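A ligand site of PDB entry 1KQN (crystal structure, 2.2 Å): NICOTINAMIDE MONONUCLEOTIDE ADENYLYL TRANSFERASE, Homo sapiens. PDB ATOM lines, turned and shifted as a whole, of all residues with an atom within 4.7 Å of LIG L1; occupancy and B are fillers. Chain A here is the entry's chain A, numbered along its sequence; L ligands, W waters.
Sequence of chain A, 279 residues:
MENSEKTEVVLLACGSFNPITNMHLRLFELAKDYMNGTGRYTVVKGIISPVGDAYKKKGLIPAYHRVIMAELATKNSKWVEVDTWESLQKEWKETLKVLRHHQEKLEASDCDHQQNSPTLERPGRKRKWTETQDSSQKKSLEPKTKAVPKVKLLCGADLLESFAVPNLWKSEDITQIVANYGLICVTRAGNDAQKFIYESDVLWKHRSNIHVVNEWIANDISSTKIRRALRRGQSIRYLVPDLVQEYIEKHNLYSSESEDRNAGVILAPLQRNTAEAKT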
ATOM      1  N   CYS A  14       6.956 -19.655   7.713  1.00  0.00           N
ATOM      2  CA  CYS A  14       7.893 -20.359   8.575  1.00  0.00           C
ATOM      3  C   CYS A  14       8.243 -21.664   7.912  1.00  0.00           C
ATOM      4  O   CYS A  14       7.366 -22.428   7.506  1.00  0.00           O
ATOM      5  CB  CYS A  14       7.283 -20.640   9.951  1.00  0.00           C
ATOM      6  SG  CYS A  14       7.139 -19.145  10.944  1.00  0.00           S
ATOM      7  N   GLY A  15       9.531 -21.945   7.789  1.00  0.00           N
ATOM      8  CA  GLY A  15       9.903 -23.187   7.150  1.00  0.00           C
ATOM      9  C   GLY A  15      11.385 -23.458   7.191  1.00  0.00           C
ATOM     10  O   GLY A  15      12.162 -22.616   7.664  1.00  0.00           O
ATOM     11  N   SER A  16      11.775 -24.625   6.704  1.00  0.00           N
ATOM     12  CA  SER A  16      13.170 -24.982   6.676  1.00  0.00           C
ATOM     13  C   SER A  16      13.968 -24.329   5.566  1.00  0.00           C
ATOM     14  O   SER A  16      15.109 -23.913   5.797  1.00  0.00           O
ATOM     15  CB  SER A  16      13.322 -26.488   6.555  1.00  0.00           C
ATOM     16  OG  SER A  16      13.070 -27.059   7.801  1.00  0.00           O
ATOM     17  N   PHE A  17      13.384 -24.261   4.373  1.00  0.00           N
ATOM     18  CA  PHE A  17      14.070 -23.666   3.199  1.00  0.00           C
ATOM     19  C   PHE A  17      15.437 -24.295   3.046  1.00  0.00           C
ATOM     20  O   PHE A  17      16.452 -23.632   3.035  1.00  0.00           O
ATOM     21  CB  PHE A  17      14.175 -22.147   3.390  1.00  0.00           C
ATOM     22  CG  PHE A  17      12.842 -21.493   3.619  1.00  0.00           C
ATOM     23  CD1 PHE A  17      12.513 -20.967   4.861  1.00  0.00           C
ATOM     24  CD2 PHE A  17      11.888 -21.448   2.585  1.00  0.00           C
ATOM     25  CE1 PHE A  17      11.256 -20.398   5.082  1.00  0.00           C
ATOM     26  CE2 PHE A  17      10.621 -20.880   2.777  1.00  0.00           C
ATOM     27  CZ  PHE A  17      10.293 -20.340   4.044  1.00  0.00           C
ATOM     28  N   ASN A  18      15.414 -25.604   2.900  1.00  0.00           N
ATOM     29  CA  ASN A  18      16.615 -26.409   2.837  1.00  0.00           C
ATOM     30  C   ASN A  18      16.710 -27.175   1.509  1.00  0.00           C
ATOM     31  O   ASN A  18      16.735 -28.404   1.507  1.00  0.00           O
ATOM     32  CB  ASN A  18      16.559 -27.400   4.026  1.00  0.00           C
ATOM     33  CG  ASN A  18      17.829 -28.231   4.163  1.00  0.00           C
ATOM     34  OD1 ASN A  18      18.917 -27.702   4.042  1.00  0.00           O
ATOM     35  ND2 ASN A  18      17.696 -29.524   4.440  1.00  0.00           N
ATOM     36  N   MET A  23       9.444 -22.648  -5.994  1.00  0.00           N
ATOM     37  CA  MET A  23       8.130 -22.934  -5.449  1.00  0.00           C
ATOM     38  C   MET A  23       7.835 -22.074  -4.216  1.00  0.00           C
ATOM     39  O   MET A  23       6.733 -21.552  -4.080  1.00  0.00           O
ATOM     40  CB  MET A  23       8.024 -24.430  -5.160  1.00  0.00           C
ATOM     41  CG  MET A  23       6.677 -24.902  -4.689  1.00  0.00           C
ATOM     42  SD  MET A  23       6.670 -24.746  -2.901  1.00  0.00           S
ATOM     43  CE  MET A  23       7.862 -26.223  -2.440  1.00  0.00           C
ATOM     44  N   HIS A  24       8.805 -21.896  -3.321  1.00  0.00           N
ATOM     45  CA  HIS A  24       8.541 -21.067  -2.130  1.00  0.00           C
ATOM     46  C   HIS A  24       8.280 -19.636  -2.581  1.00  0.00           C
ATOM     47  O   HIS A  24       7.467 -18.941  -1.970  1.00  0.00           O
ATOM     48  CB  HIS A  24       9.750 -21.051  -1.175  1.00  0.00           C
ATOM     49  CG  HIS A  24      10.100 -22.389  -0.599  1.00  0.00           C
ATOM     50  ND1 HIS A  24      11.213 -23.102  -0.978  1.00  0.00           N
ATOM     51  CD2 HIS A  24       9.424 -23.182   0.275  1.00  0.00           C
ATOM     52  CE1 HIS A  24      11.210 -24.285  -0.385  1.00  0.00           C
ATOM     53  NE2 HIS A  24      10.130 -24.362   0.379  1.00  0.00           N
ATOM     54  N   LEU A  27       4.781 -19.272  -3.997  1.00  0.00           N
ATOM     55  CA  LEU A  27       3.867 -19.292  -2.881  1.00  0.00           C
ATOM     56  C   LEU A  27       3.478 -17.907  -2.453  1.00  0.00           C
ATOM     57  O   LEU A  27       2.322 -17.632  -2.207  1.00  0.00           O
ATOM     58  CB  LEU A  27       4.527 -19.959  -1.702  1.00  0.00           C
ATOM     59  CG  LEU A  27       3.594 -20.802  -0.877  1.00  0.00           C
ATOM     60  CD1 LEU A  27       3.151 -21.949  -1.741  1.00  0.00           C
ATOM     61  CD2 LEU A  27       4.325 -21.302   0.368  1.00  0.00           C
ATOM     62  N   VAL A  51      14.076 -21.760   9.805  1.00  0.00           N
ATOM     63  CA  VAL A  51      14.089 -22.314  11.141  1.00  0.00           C
ATOM     64  C   VAL A  51      15.541 -22.472  11.678  1.00  0.00           C
ATOM     65  O   VAL A  51      16.466 -22.737  10.925  1.00  0.00           O
ATOM     66  CB  VAL A  51      13.336 -23.649  11.121  1.00  0.00           C
ATOM     67  CG1 VAL A  51      14.181 -24.732  10.436  1.00  0.00           C
ATOM     68  CG2 VAL A  51      12.913 -24.038  12.535  1.00  0.00           C
ATOM     69  N   TYR A  55      15.824 -27.074  15.441  1.00  0.00           N
ATOM     70  CA  TYR A  55      14.606 -27.750  15.004  1.00  0.00           C
ATOM     71  C   TYR A  55      15.030 -29.201  14.851  1.00  0.00           C
ATOM     72  O   TYR A  55      14.256 -30.127  15.161  1.00  0.00           O
ATOM     73  CB  TYR A  55      14.078 -27.155  13.695  1.00  0.00           C
ATOM     74  CG  TYR A  55      12.781 -27.760  13.152  1.00  0.00           C
ATOM     75  CD1 TYR A  55      11.619 -27.808  13.940  1.00  0.00           C
ATOM     76  CD2 TYR A  55      12.711 -28.257  11.844  1.00  0.00           C
ATOM     77  CE1 TYR A  55      10.434 -28.347  13.428  1.00  0.00           C
ATOM     78  CE2 TYR A  55      11.541 -28.779  11.334  1.00  0.00           C
ATOM     79  CZ  TYR A  55      10.414 -28.817  12.125  1.00  0.00           C
ATOM     80  OH  TYR A  55       9.254 -29.279  11.577  1.00  0.00           O
ATOM     81  N   LYS A  57      15.717 -31.083  12.180  1.00  0.00           N
ATOM     82  CA  LYS A  57      15.183 -31.889  11.085  1.00  0.00           C
ATOM     83  C   LYS A  57      16.285 -32.669  10.336  1.00  0.00           C
ATOM     84  O   LYS A  57      17.396 -32.175  10.152  1.00  0.00           O
ATOM     85  CB  LYS A  57      14.443 -30.955  10.097  1.00  0.00           C
ATOM     86  CG  LYS A  57      13.827 -31.626   8.853  1.00  0.00           C
ATOM     87  CD  LYS A  57      13.113 -30.539   7.996  1.00  0.00           C
ATOM     88  CE  LYS A  57      12.226 -31.135   6.914  1.00  0.00           C
ATOM     89  NZ  LYS A  57      11.614 -30.062   6.076  1.00  0.00           N
ATOM     90  N   GLU A  86      14.240 -16.326  14.052  1.00  0.00           N
ATOM     91  CA  GLU A  86      14.092 -17.721  14.289  1.00  0.00           C
ATOM     92  C   GLU A  86      15.408 -18.494  14.081  1.00  0.00           C
ATOM     93  O   GLU A  86      15.715 -19.437  14.846  1.00  0.00           O
ATOM     94  CB  GLU A  86      12.958 -18.165  13.366  1.00  0.00           C
ATOM     95  CG  GLU A  86      12.365 -19.485  13.708  1.00  0.00           C
ATOM     96  CD  GLU A  86      11.082 -19.821  12.966  1.00  0.00           C
ATOM     97  OE1 GLU A  86      10.634 -20.964  13.191  1.00  0.00           O
ATOM     98  OE2 GLU A  86      10.517 -19.003  12.193  1.00  0.00           O
ATOM     99  N   TRP A  92      14.638 -24.250  19.830  1.00  0.00           N
ATOM    100  CA  TRP A  92      13.657 -24.168  18.762  1.00  0.00           C
ATOM    101  C   TRP A  92      12.375 -23.462  19.245  1.00  0.00           C
ATOM    102  O   TRP A  92      11.856 -23.720  20.326  1.00  0.00           O
ATOM    103  CB  TRP A  92      13.371 -25.565  18.250  1.00  0.00           C
ATOM    104  CG  TRP A  92      12.201 -25.600  17.321  1.00  0.00           C
ATOM    105  CD1 TRP A  92      12.176 -25.199  16.014  1.00  0.00           C
ATOM    106  CD2 TRP A  92      10.871 -25.972  17.667  1.00  0.00           C
ATOM    107  NE1 TRP A  92      10.896 -25.297  15.525  1.00  0.00           N
ATOM    108  CE2 TRP A  92      10.072 -25.764  16.520  1.00  0.00           C
ATOM    109  CE3 TRP A  92      10.273 -26.453  18.840  1.00  0.00           C
ATOM    110  CZ2 TRP A  92       8.698 -26.013  16.503  1.00  0.00           C
ATOM    111  CZ3 TRP A  92       8.911 -26.707  18.829  1.00  0.00           C
ATOM    112  CH2 TRP A  92       8.131 -26.479  17.661  1.00  0.00           C
ATOM    113  N   LYS A  93      11.882 -22.520  18.448  1.00  0.00           N
ATOM    114  CA  LYS A  93      10.673 -21.775  18.812  1.00  0.00           C
ATOM    115  C   LYS A  93       9.383 -22.285  18.090  1.00  0.00           C
ATOM    116  O   LYS A  93       9.408 -22.556  16.883  1.00  0.00           O
ATOM    117  CB  LYS A  93      10.898 -20.299  18.502  1.00  0.00           C
ATOM    118  CG  LYS A  93      11.031 -19.367  19.706  1.00  0.00           C
ATOM    119  CD  LYS A  93      11.931 -19.940  20.777  1.00  0.00           C
ATOM    120  CE  LYS A  93      12.116 -18.999  21.969  1.00  0.00           C
ATOM    121  NZ  LYS A  93      13.040 -19.706  22.944  1.00  0.00           N
ATOM    122  N   GLU A  94       8.296 -22.432  18.843  1.00  0.00           N
ATOM    123  CA  GLU A  94       6.996 -22.861  18.283  1.00  0.00           C
ATOM    124  C   GLU A  94       6.486 -21.784  17.306  1.00  0.00           C
ATOM    125  O   GLU A  94       6.584 -20.575  17.592  1.00  0.00           O
ATOM    126  CB  GLU A  94       5.928 -23.024  19.387  1.00  0.00           C
ATOM    127  CG  GLU A  94       5.996 -24.318  20.174  1.00  0.00           C
ATOM    128  CD  GLU A  94       7.017 -24.304  21.327  1.00  0.00           C
ATOM    129  OE1 GLU A  94       7.721 -23.279  21.533  1.00  0.00           O
ATOM    130  OE2 GLU A  94       7.108 -25.338  22.029  1.00  0.00           O
ATOM    131  N   THR A  95       5.920 -22.207  16.173  1.00  0.00           N
ATOM    132  CA  THR A  95       5.411 -21.240  15.203  1.00  0.00           C
ATOM    133  C   THR A  95       4.485 -20.199  15.810  1.00  0.00           C
ATOM    134  O   THR A  95       4.483 -19.022  15.381  1.00  0.00           O
ATOM    135  CB  THR A  95       4.690 -21.918  14.032  1.00  0.00           C
ATOM    136  OG1 THR A  95       5.610 -22.806  13.378  1.00  0.00           O
ATOM    137  CG2 THR A  95       4.173 -20.850  13.010  1.00  0.00           C
ATOM    138  N   LEU A  96       3.675 -20.612  16.785  1.00  0.00           N
ATOM    139  CA  LEU A  96       2.791 -19.647  17.432  1.00  0.00           C
ATOM    140  C   LEU A  96       3.658 -18.536  18.055  1.00  0.00           C
ATOM    141  O   LEU A  96       3.297 -17.341  17.994  1.00  0.00           O
ATOM    142  CB  LEU A  96       1.904 -20.326  18.495  1.00  0.00           C
ATOM    143  CG  LEU A  96       1.081 -19.354  19.388  1.00  0.00           C
ATOM    144  CD1 LEU A  96       0.145 -18.439  18.585  1.00  0.00           C
ATOM    145  CD2 LEU A  96       0.310 -20.186  20.409  1.00  0.00           C
ATOM    146  N   LEU A 154       1.710 -18.217   6.145  1.00  0.00           N
ATOM    147  CA  LEU A 154       1.621 -18.642   4.746  1.00  0.00           C
ATOM    148  C   LEU A 154       2.174 -20.051   4.743  1.00  0.00           C
ATOM    149  O   LEU A 154       3.290 -20.256   5.225  1.00  0.00           O
ATOM    150  CB  LEU A 154       2.564 -17.806   3.894  1.00  0.00           C
ATOM    151  CG  LEU A 154       2.227 -17.519   2.424  1.00  0.00           C
ATOM    152  CD1 LEU A 154       3.503 -17.275   1.657  1.00  0.00           C
ATOM    153  CD2 LEU A 154       1.429 -18.657   1.826  1.00  0.00           C
ATOM    154  N   CYS A 155       1.459 -21.015   4.211  1.00  0.00           N
ATOM    155  CA  CYS A 155       1.988 -22.346   4.186  1.00  0.00           C
ATOM    156  C   CYS A 155       1.318 -23.134   3.095  1.00  0.00           C
ATOM    157  O   CYS A 155       0.489 -22.615   2.335  1.00  0.00           O
ATOM    158  CB  CYS A 155       1.714 -23.029   5.523  1.00  0.00           C
ATOM    159  SG  CYS A 155      -0.067 -23.166   5.810  1.00  0.00           S
ATOM    160  N   GLY A 156       1.702 -24.413   3.033  1.00  0.00           N
ATOM    161  CA  GLY A 156       1.142 -25.343   2.081  1.00  0.00           C
ATOM    162  C   GLY A 156       0.253 -26.339   2.819  1.00  0.00           C
ATOM    163  O   GLY A 156       0.152 -26.344   4.066  1.00  0.00           O
ATOM    164  N   ALA A 157      -0.378 -27.219   2.058  1.00  0.00           N
ATOM    165  CA  ALA A 157      -1.269 -28.229   2.595  1.00  0.00           C
ATOM    166  C   ALA A 157      -0.553 -29.153   3.571  1.00  0.00           C
ATOM    167  O   ALA A 157      -1.159 -29.601   4.528  1.00  0.00           O
ATOM    168  CB  ALA A 157      -1.880 -29.067   1.458  1.00  0.00           C
ATOM    169  N   ASP A 158       0.725 -29.457   3.290  1.00  0.00           N
ATOM    170  CA  ASP A 158       1.535 -30.311   4.130  1.00  0.00           C
ATOM    171  C   ASP A 158       1.629 -29.794   5.547  1.00  0.00           C
ATOM    172  O   ASP A 158       1.507 -30.551   6.516  1.00  0.00           O
ATOM    173  CB  ASP A 158       2.951 -30.420   3.586  1.00  0.00           C
ATOM    174  CG  ASP A 158       3.135 -31.648   2.724  1.00  0.00           C
ATOM    175  OD1 ASP A 158       2.278 -31.914   1.831  1.00  0.00           O
ATOM    176  OD2 ASP A 158       4.148 -32.364   2.923  1.00  0.00           O
ATOM    177  N   LEU A 159       1.859 -28.497   5.702  1.00  0.00           N
ATOM    178  CA  LEU A 159       1.978 -27.963   7.062  1.00  0.00           C
ATOM    179  C   LEU A 159       0.617 -28.014   7.756  1.00  0.00           C
ATOM    180  O   LEU A 159       0.516 -28.408   8.927  1.00  0.00           O
ATOM    181  CB  LEU A 159       2.565 -26.527   7.046  1.00  0.00           C
ATOM    182  CG  LEU A 159       2.946 -25.852   8.385  1.00  0.00           C
ATOM    183  CD1 LEU A 159       4.025 -24.796   8.180  1.00  0.00           C
ATOM    184  CD2 LEU A 159       1.709 -25.225   9.004  1.00  0.00           C
ATOM    185  N   LEU A 168       2.931 -33.312  17.428  1.00  0.00           N
ATOM    186  CA  LEU A 168       3.691 -32.321  16.695  1.00  0.00           C
ATOM    187  C   LEU A 168       3.324 -30.911  17.080  1.00  0.00           C
ATOM    188  O   LEU A 168       4.187 -30.038  17.187  1.00  0.00           O
ATOM    189  CB  LEU A 168       3.517 -32.546  15.191  1.00  0.00           C
ATOM    190  CG  LEU A 168       4.456 -31.813  14.240  1.00  0.00           C
ATOM    191  CD1 LEU A 168       5.907 -32.212  14.532  1.00  0.00           C
ATOM    192  CD2 LEU A 168       4.117 -32.182  12.782  1.00  0.00           C
ATOM    193  N   TRP A 169       2.046 -30.675  17.284  1.00  0.00           N
ATOM    194  CA  TRP A 169       1.573 -29.367  17.646  1.00  0.00           C
ATOM    195  C   TRP A 169       0.701 -29.432  18.899  1.00  0.00           C
ATOM    196  O   TRP A 169      -0.209 -30.271  18.972  1.00  0.00           O
ATOM    197  CB  TRP A 169       0.695 -28.799  16.523  1.00  0.00           C
ATOM    198  CG  TRP A 169       1.355 -28.647  15.177  1.00  0.00           C
ATOM    199  CD1 TRP A 169       1.633 -29.632  14.258  1.00  0.00           C
ATOM    200  CD2 TRP A 169       1.807 -27.419  14.594  1.00  0.00           C
ATOM    201  NE1 TRP A 169       2.233 -29.079  13.141  1.00  0.00           N
ATOM    202  CE2 TRP A 169       2.345 -27.720  13.320  1.00  0.00           C
ATOM    203  CE3 TRP A 169       1.789 -26.082  15.024  1.00  0.00           C
ATOM    204  CZ2 TRP A 169       2.863 -26.736  12.471  1.00  0.00           C
ATOM    205  CZ3 TRP A 169       2.314 -25.104  14.193  1.00  0.00           C
ATOM    206  CH2 TRP A 169       2.846 -25.437  12.922  1.00  0.00           C
ATOM    207  N   ASP A 173      -2.031 -24.534  20.588  1.00  0.00           N
ATOM    208  CA  ASP A 173      -1.242 -23.775  19.625  1.00  0.00           C
ATOM    209  C   ASP A 173      -2.070 -23.730  18.345  1.00  0.00           C
ATOM    210  O   ASP A 173      -2.307 -22.665  17.785  1.00  0.00           O
ATOM    211  CB  ASP A 173       0.115 -24.439  19.408  1.00  0.00           C
ATOM    212  CG  ASP A 173       1.197 -23.975  20.441  1.00  0.00           C
ATOM    213  OD1 ASP A 173       0.873 -23.233  21.402  1.00  0.00           O
ATOM    214  OD2 ASP A 173       2.382 -24.366  20.280  1.00  0.00           O
ATOM    215  N   VAL A 186      -1.741 -22.541   0.547  1.00  0.00           N
ATOM    216  CA  VAL A 186      -1.665 -22.687  -0.886  1.00  0.00           C
ATOM    217  C   VAL A 186      -1.482 -24.145  -1.242  1.00  0.00           C
ATOM    218  O   VAL A 186      -0.607 -24.827  -0.705  1.00  0.00           O
ATOM    219  CB  VAL A 186      -0.491 -21.881  -1.456  1.00  0.00           C
ATOM    220  CG1 VAL A 186      -0.431 -22.076  -2.933  1.00  0.00           C
ATOM    221  CG2 VAL A 186      -0.661 -20.409  -1.131  1.00  0.00           C
ATOM    222  N   GLU A 215      -3.749 -23.699  -6.451  1.00  0.00           N
ATOM    223  CA  GLU A 215      -2.546 -23.532  -7.254  1.00  0.00           C
ATOM    224  C   GLU A 215      -2.874 -24.296  -8.551  1.00  0.00           C
ATOM    225  O   GLU A 215      -2.653 -25.495  -8.657  1.00  0.00           O
ATOM    226  CB  GLU A 215      -1.366 -24.183  -6.470  1.00  0.00           C
ATOM    227  CG  GLU A 215       0.006 -24.405  -7.159  1.00  0.00           C
ATOM    228  CD  GLU A 215       0.962 -25.297  -6.255  1.00  0.00           C
ATOM    229  OE1 GLU A 215       0.943 -25.148  -4.993  1.00  0.00           O
ATOM    230  OE2 GLU A 215       1.750 -26.130  -6.796  1.00  0.00           O
ATOM    231  N   ASN A 219       2.959 -27.082  -9.259  1.00  0.00           N
ATOM    232  CA  ASN A 219       4.347 -26.794  -8.937  1.00  0.00           C
ATOM    233  C   ASN A 219       4.653 -27.726  -7.773  1.00  0.00           C
ATOM    234  O   ASN A 219       3.894 -27.761  -6.785  1.00  0.00           O
ATOM    235  CB  ASN A 219       4.369 -25.302  -8.489  1.00  0.00           C
ATOM    236  CG  ASN A 219       5.737 -24.801  -8.046  1.00  0.00           C
ATOM    237  OD1 ASN A 219       5.873 -23.618  -7.702  1.00  0.00           O
ATOM    238  ND2 ASN A 219       6.756 -25.682  -8.058  1.00  0.00           N
ATOM    239  N   ASP A 220       5.701 -28.524  -7.897  1.00  0.00           N
ATOM    240  CA  ASP A 220       6.079 -29.350  -6.774  1.00  0.00           C
ATOM    241  C   ASP A 220       7.583 -29.498  -6.743  1.00  0.00           C
ATOM    242  O   ASP A 220       8.159 -30.591  -6.746  1.00  0.00           O
ATOM    243  CB  ASP A 220       5.303 -30.680  -6.741  1.00  0.00           C
ATOM    244  CG  ASP A 220       6.052 -31.842  -7.379  1.00  0.00           C
ATOM    245  OD1 ASP A 220       6.257 -31.817  -8.619  1.00  0.00           O
ATOM    246  OD2 ASP A 220       6.417 -32.787  -6.632  1.00  0.00           O
ATOM    247  N   SER A 223      12.146 -29.119  -1.759  1.00  0.00           N
ATOM    248  CA  SER A 223      13.532 -29.043  -1.354  1.00  0.00           C
ATOM    249  C   SER A 223      14.118 -30.463  -1.436  1.00  0.00           C
ATOM    250  O   SER A 223      15.226 -30.644  -1.922  1.00  0.00           O
ATOM    251  CB  SER A 223      13.634 -28.547   0.098  1.00  0.00           C
ATOM    252  OG  SER A 223      13.274 -27.172   0.173  1.00  0.00           O
ATOM    253  N   PRO A 269       9.919 -30.302  18.089  1.00  0.00           N
ATOM    254  CA  PRO A 269       8.552 -30.297  18.648  1.00  0.00           C
ATOM    255  C   PRO A 269       8.131 -31.638  19.261  1.00  0.00           C
ATOM    256  O   PRO A 269       7.554 -31.646  20.311  1.00  0.00           O
ATOM    257  CB  PRO A 269       7.673 -29.926  17.459  1.00  0.00           C
ATOM    258  CG  PRO A 269       8.652 -29.378  16.423  1.00  0.00           C
ATOM    259  CD  PRO A 269       9.903 -30.126  16.638  1.00  0.00           C
HETATM  260  P1  LIG L   1       9.718 -26.260   4.061  1.00  0.00           P
HETATM  261  O1  LIG L   1      10.859 -25.368   3.705  1.00  0.00           O
HETATM  262  O2  LIG L   1       9.877 -27.609   3.463  1.00  0.00           O
HETATM  263  O3  LIG L   1       8.322 -25.662   3.456  1.00  0.00           O
HETATM  264  C1  LIG L   1       7.945 -24.246   3.606  1.00  0.00           C
HETATM  265  C2  LIG L   1       6.478 -24.191   3.203  1.00  0.00           C
HETATM  266  O4  LIG L   1       6.259 -24.610   1.802  1.00  0.00           O
HETATM  267  C3  LIG L   1       5.543 -25.111   4.036  1.00  0.00           C
HETATM  268  O5  LIG L   1       4.502 -24.353   4.671  1.00  0.00           O
HETATM  269  C4  LIG L   1       5.068 -26.115   2.977  1.00  0.00           C
HETATM  270  O6  LIG L   1       3.779 -26.731   3.306  1.00  0.00           O
HETATM  271  C5  LIG L   1       5.047 -25.230   1.699  1.00  0.00           C
HETATM  272  N1  LIG L   1       5.054 -26.010   0.493  1.00  0.00           N
HETATM  273  C6  LIG L   1       5.878 -27.031   0.153  1.00  0.00           C
HETATM  274  N2  LIG L   1       5.618 -27.570  -1.056  1.00  0.00           N
HETATM  275  C7  LIG L   1       4.561 -26.818  -1.482  1.00  0.00           C
HETATM  276  C8  LIG L   1       3.795 -26.862  -2.691  1.00  0.00           C
HETATM  277  N3  LIG L   1       4.007 -27.700  -3.694  1.00  0.00           N
HETATM  278  N4  LIG L   1       2.768 -25.965  -2.825  1.00  0.00           N
HETATM  279  C9  LIG L   1       2.528 -25.079  -1.808  1.00  0.00           C
HETATM  280  N5  LIG L   1       3.177 -24.963  -0.661  1.00  0.00           N
HETATM  281  C10 LIG L   1       4.183 -25.859  -0.553  1.00  0.00           C
HETATM  282  O7  LIG L   1       9.569 -26.240   5.660  1.00  0.00           O
HETATM  283  P2  LIG L   1       9.093 -27.399   6.691  1.00  0.00           P
HETATM  284  O8  LIG L   1      10.152 -28.273   7.218  1.00  0.00           O
HETATM  285  O9  LIG L   1       7.997 -28.219   6.080  1.00  0.00           O
HETATM  286  O10 LIG L   1       8.652 -26.345   7.748  1.00  0.00           O
HETATM  287  C11 LIG L   1       8.298 -26.706   9.095  1.00  0.00           C
HETATM  288  C12 LIG L   1       7.904 -25.420   9.711  1.00  0.00           C
HETATM  289  O11 LIG L   1       6.767 -25.747  10.518  1.00  0.00           O
HETATM  290  C13 LIG L   1       8.947 -24.776  10.630  1.00  0.00           C
HETATM  291  O12 LIG L   1       8.735 -23.345  10.690  1.00  0.00           O
HETATM  292  C14 LIG L   1       8.598 -25.384  11.926  1.00  0.00           C
HETATM  293  O13 LIG L   1       9.180 -24.689  13.068  1.00  0.00           O
HETATM  294  C15 LIG L   1       7.049 -25.361  11.845  1.00  0.00           C
HETATM  295  N6  LIG L   1       6.490 -26.305  12.797  1.00  0.00           N
HETATM  296  C16 LIG L   1       5.988 -25.840  14.016  1.00  0.00           C
HETATM  297  C17 LIG L   1       5.449 -26.742  14.997  1.00  0.00           C
HETATM  298  C18 LIG L   1       4.958 -26.092  16.231  1.00  0.00           C
HETATM  299  O14 LIG L   1       4.506 -26.889  17.067  1.00  0.00           O
HETATM  300  N7  LIG L   1       4.999 -24.738  16.430  1.00  0.00           N
HETATM  301  C19 LIG L   1       5.430 -28.200  14.713  1.00  0.00           C
HETATM  302  C20 LIG L   1       5.984 -28.631  13.380  1.00  0.00           C
HETATM  303  C21 LIG L   1       6.467 -27.712  12.531  1.00  0.00           C
HETATM  304 XE1  LG2 L   2       3.471 -22.771  -5.054  1.00  0.00          XE
HETATM  305  O   HOH W   1      12.982 -26.730   2.637  1.00  0.00           O
HETATM  306  O   HOH W   2      10.831 -21.581  10.511  1.00  0.00           O
HETATM  307  O   HOH W   3       9.349 -30.475   9.326  1.00  0.00           O
HETATM  308  O   HOH W   4       2.726 -28.470   1.486  1.00  0.00           O
HETATM  309  O   HOH W   5       8.505 -22.415  13.891  1.00  0.00           O
HETATM  310  O   HOH W   6       9.975 -27.535   0.484  1.00  0.00           O
HETATM  311  O   HOH W   7       3.072 -23.283  17.447  1.00  0.00           O
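The backbone NH (N) of Gly 15 sits at hydrogen-bond distance from an oxygen (O12) of LIG L1 (3.3 Å). The side-chain hydroxyl of Ser 16 is in hydrogen-bond range of an oxygen (O8) of LIG L1 (3.2 Å). O of Asn 219 lies within hydrogen-bond range of N3 of LIG L1 (3.1 Å). N7 of LIG L1 lies close to N of Thr 95 (2.7 Å). N of Gly 156 lies within hydrogen-bond range of O6 of LIG L1 (3.1 Å). NE1 of Trp 92 lies within hydrogen-bond range of O13 of LIG L1. An oxygen (O1) of LIG L1 sits at hydrogen-bond distance from the backbone NH of Phe 17, 2.8 Å away. An oxygen (O7) of LIG L1 is in hydrogen-bond range of the backbone NH (N) of Ser 16 (2.9 Å). O8 of LIG L1 lies within salt-bridge range of NZ of Lys 57 (2.6 Å).
OE2 of Glu 86 sits at hydrogen-bond distance from SG of Cys 14, 3.6 Å away. O of Gly 15 sits at hydrogen-bond distance from N of Val 51, at 3.0 Å. OE2 of Glu 215 is in hydrogen-bond range of N of Asn 219 (2.9 Å). The backbone carbonyl oxygen of Cys 155 is in hydrogen-bond range of the backbone NH of Val 186 (2.9 Å).
SD of Met 23 sits close to N2 of LIG L1. An oxygen (O14) of LIG L1 lies close to the backbone carbonyl oxygen of Leu 168. The side-chain carboxylate of Glu 215 lies close to a nitrogen (N4) of LIG L1. Merely in contact with LIG L1: Cys 14 (3.2 Å), His 24 (3.6 Å), Leu 27 (3.2 Å), Val 51 (3.8 Å), Tyr 55 (3.3 Å), Glu 86 (3.9 Å), Glu 94 (3.3 Å), Cys 155 (3.2 Å), Asp 158 (3.8 Å), Leu 159 (3.5 Å), Trp 169 (3.4 Å), Val 186 (3.3 Å) and Pro 269 (3.8 Å). Hydrophobic or aromatic side chains that line LIG L1: Met 23, His 24, Leu 27, Val 51, Tyr 55, Trp 92, Leu 159, Leu 168, Trp 169 and Pro 269. 24 residues have an atom within 4 Å of LIG L1: Cys 14, Gly 15, Ser 16, Phe 17, Met 23, His 24, Leu 27, Val 51, Tyr 55, Lys 57, Glu 86, Trp 92, Glu 94, Thr 95, Cys 155, Gly 156, Asp 158, Leu 159, Leu 168, Trp 169, Val 186, Glu 215, Asn 219 and Pro 269.
Water W5 lies within hydrogen-bond range of an oxygen (O13) of LIG L1 (2.5 Å), the side-chain carboxylate of Glu 86 (2.7 Å), the side-chain hydroxyl of Thr 95 (3.0 Å) and the backbone carbonyl oxygen of Lys 93 (3.1 Å). Water W4 lies within hydrogen-bond range of O6 of LIG L1, N of Asp 158 and N of Ala 157. Water W1 lies within hydrogen-bond range of OG of Ser 223 (2.5 Å), N of Asn 18 (2.7 Å), O1 of LIG L1 (2.7 Å) and N of Phe 17 (3.0 Å). Water W2 lies within hydrogen-bond range of O12 of LIG L1 (2.7 Å), OE1 of Glu 86 (2.8 Å), N of Gly 15 (3.0 Å) and N of Val 51 (3.3 Å). Water W6 lies within hydrogen-bond range of an oxygen (O2) of LIG L1 (3.0 Å), a ring nitrogen (NE2) of His 24 (3.2 Å) and the side-chain hydroxyl (OG) of Ser 223 (3.3 Å). Water W3 bridges the side-chain hydroxyl (OH) of Tyr 55 (2.6 Å) and an oxygen (O8) of LIG L1 (3.2 Å).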
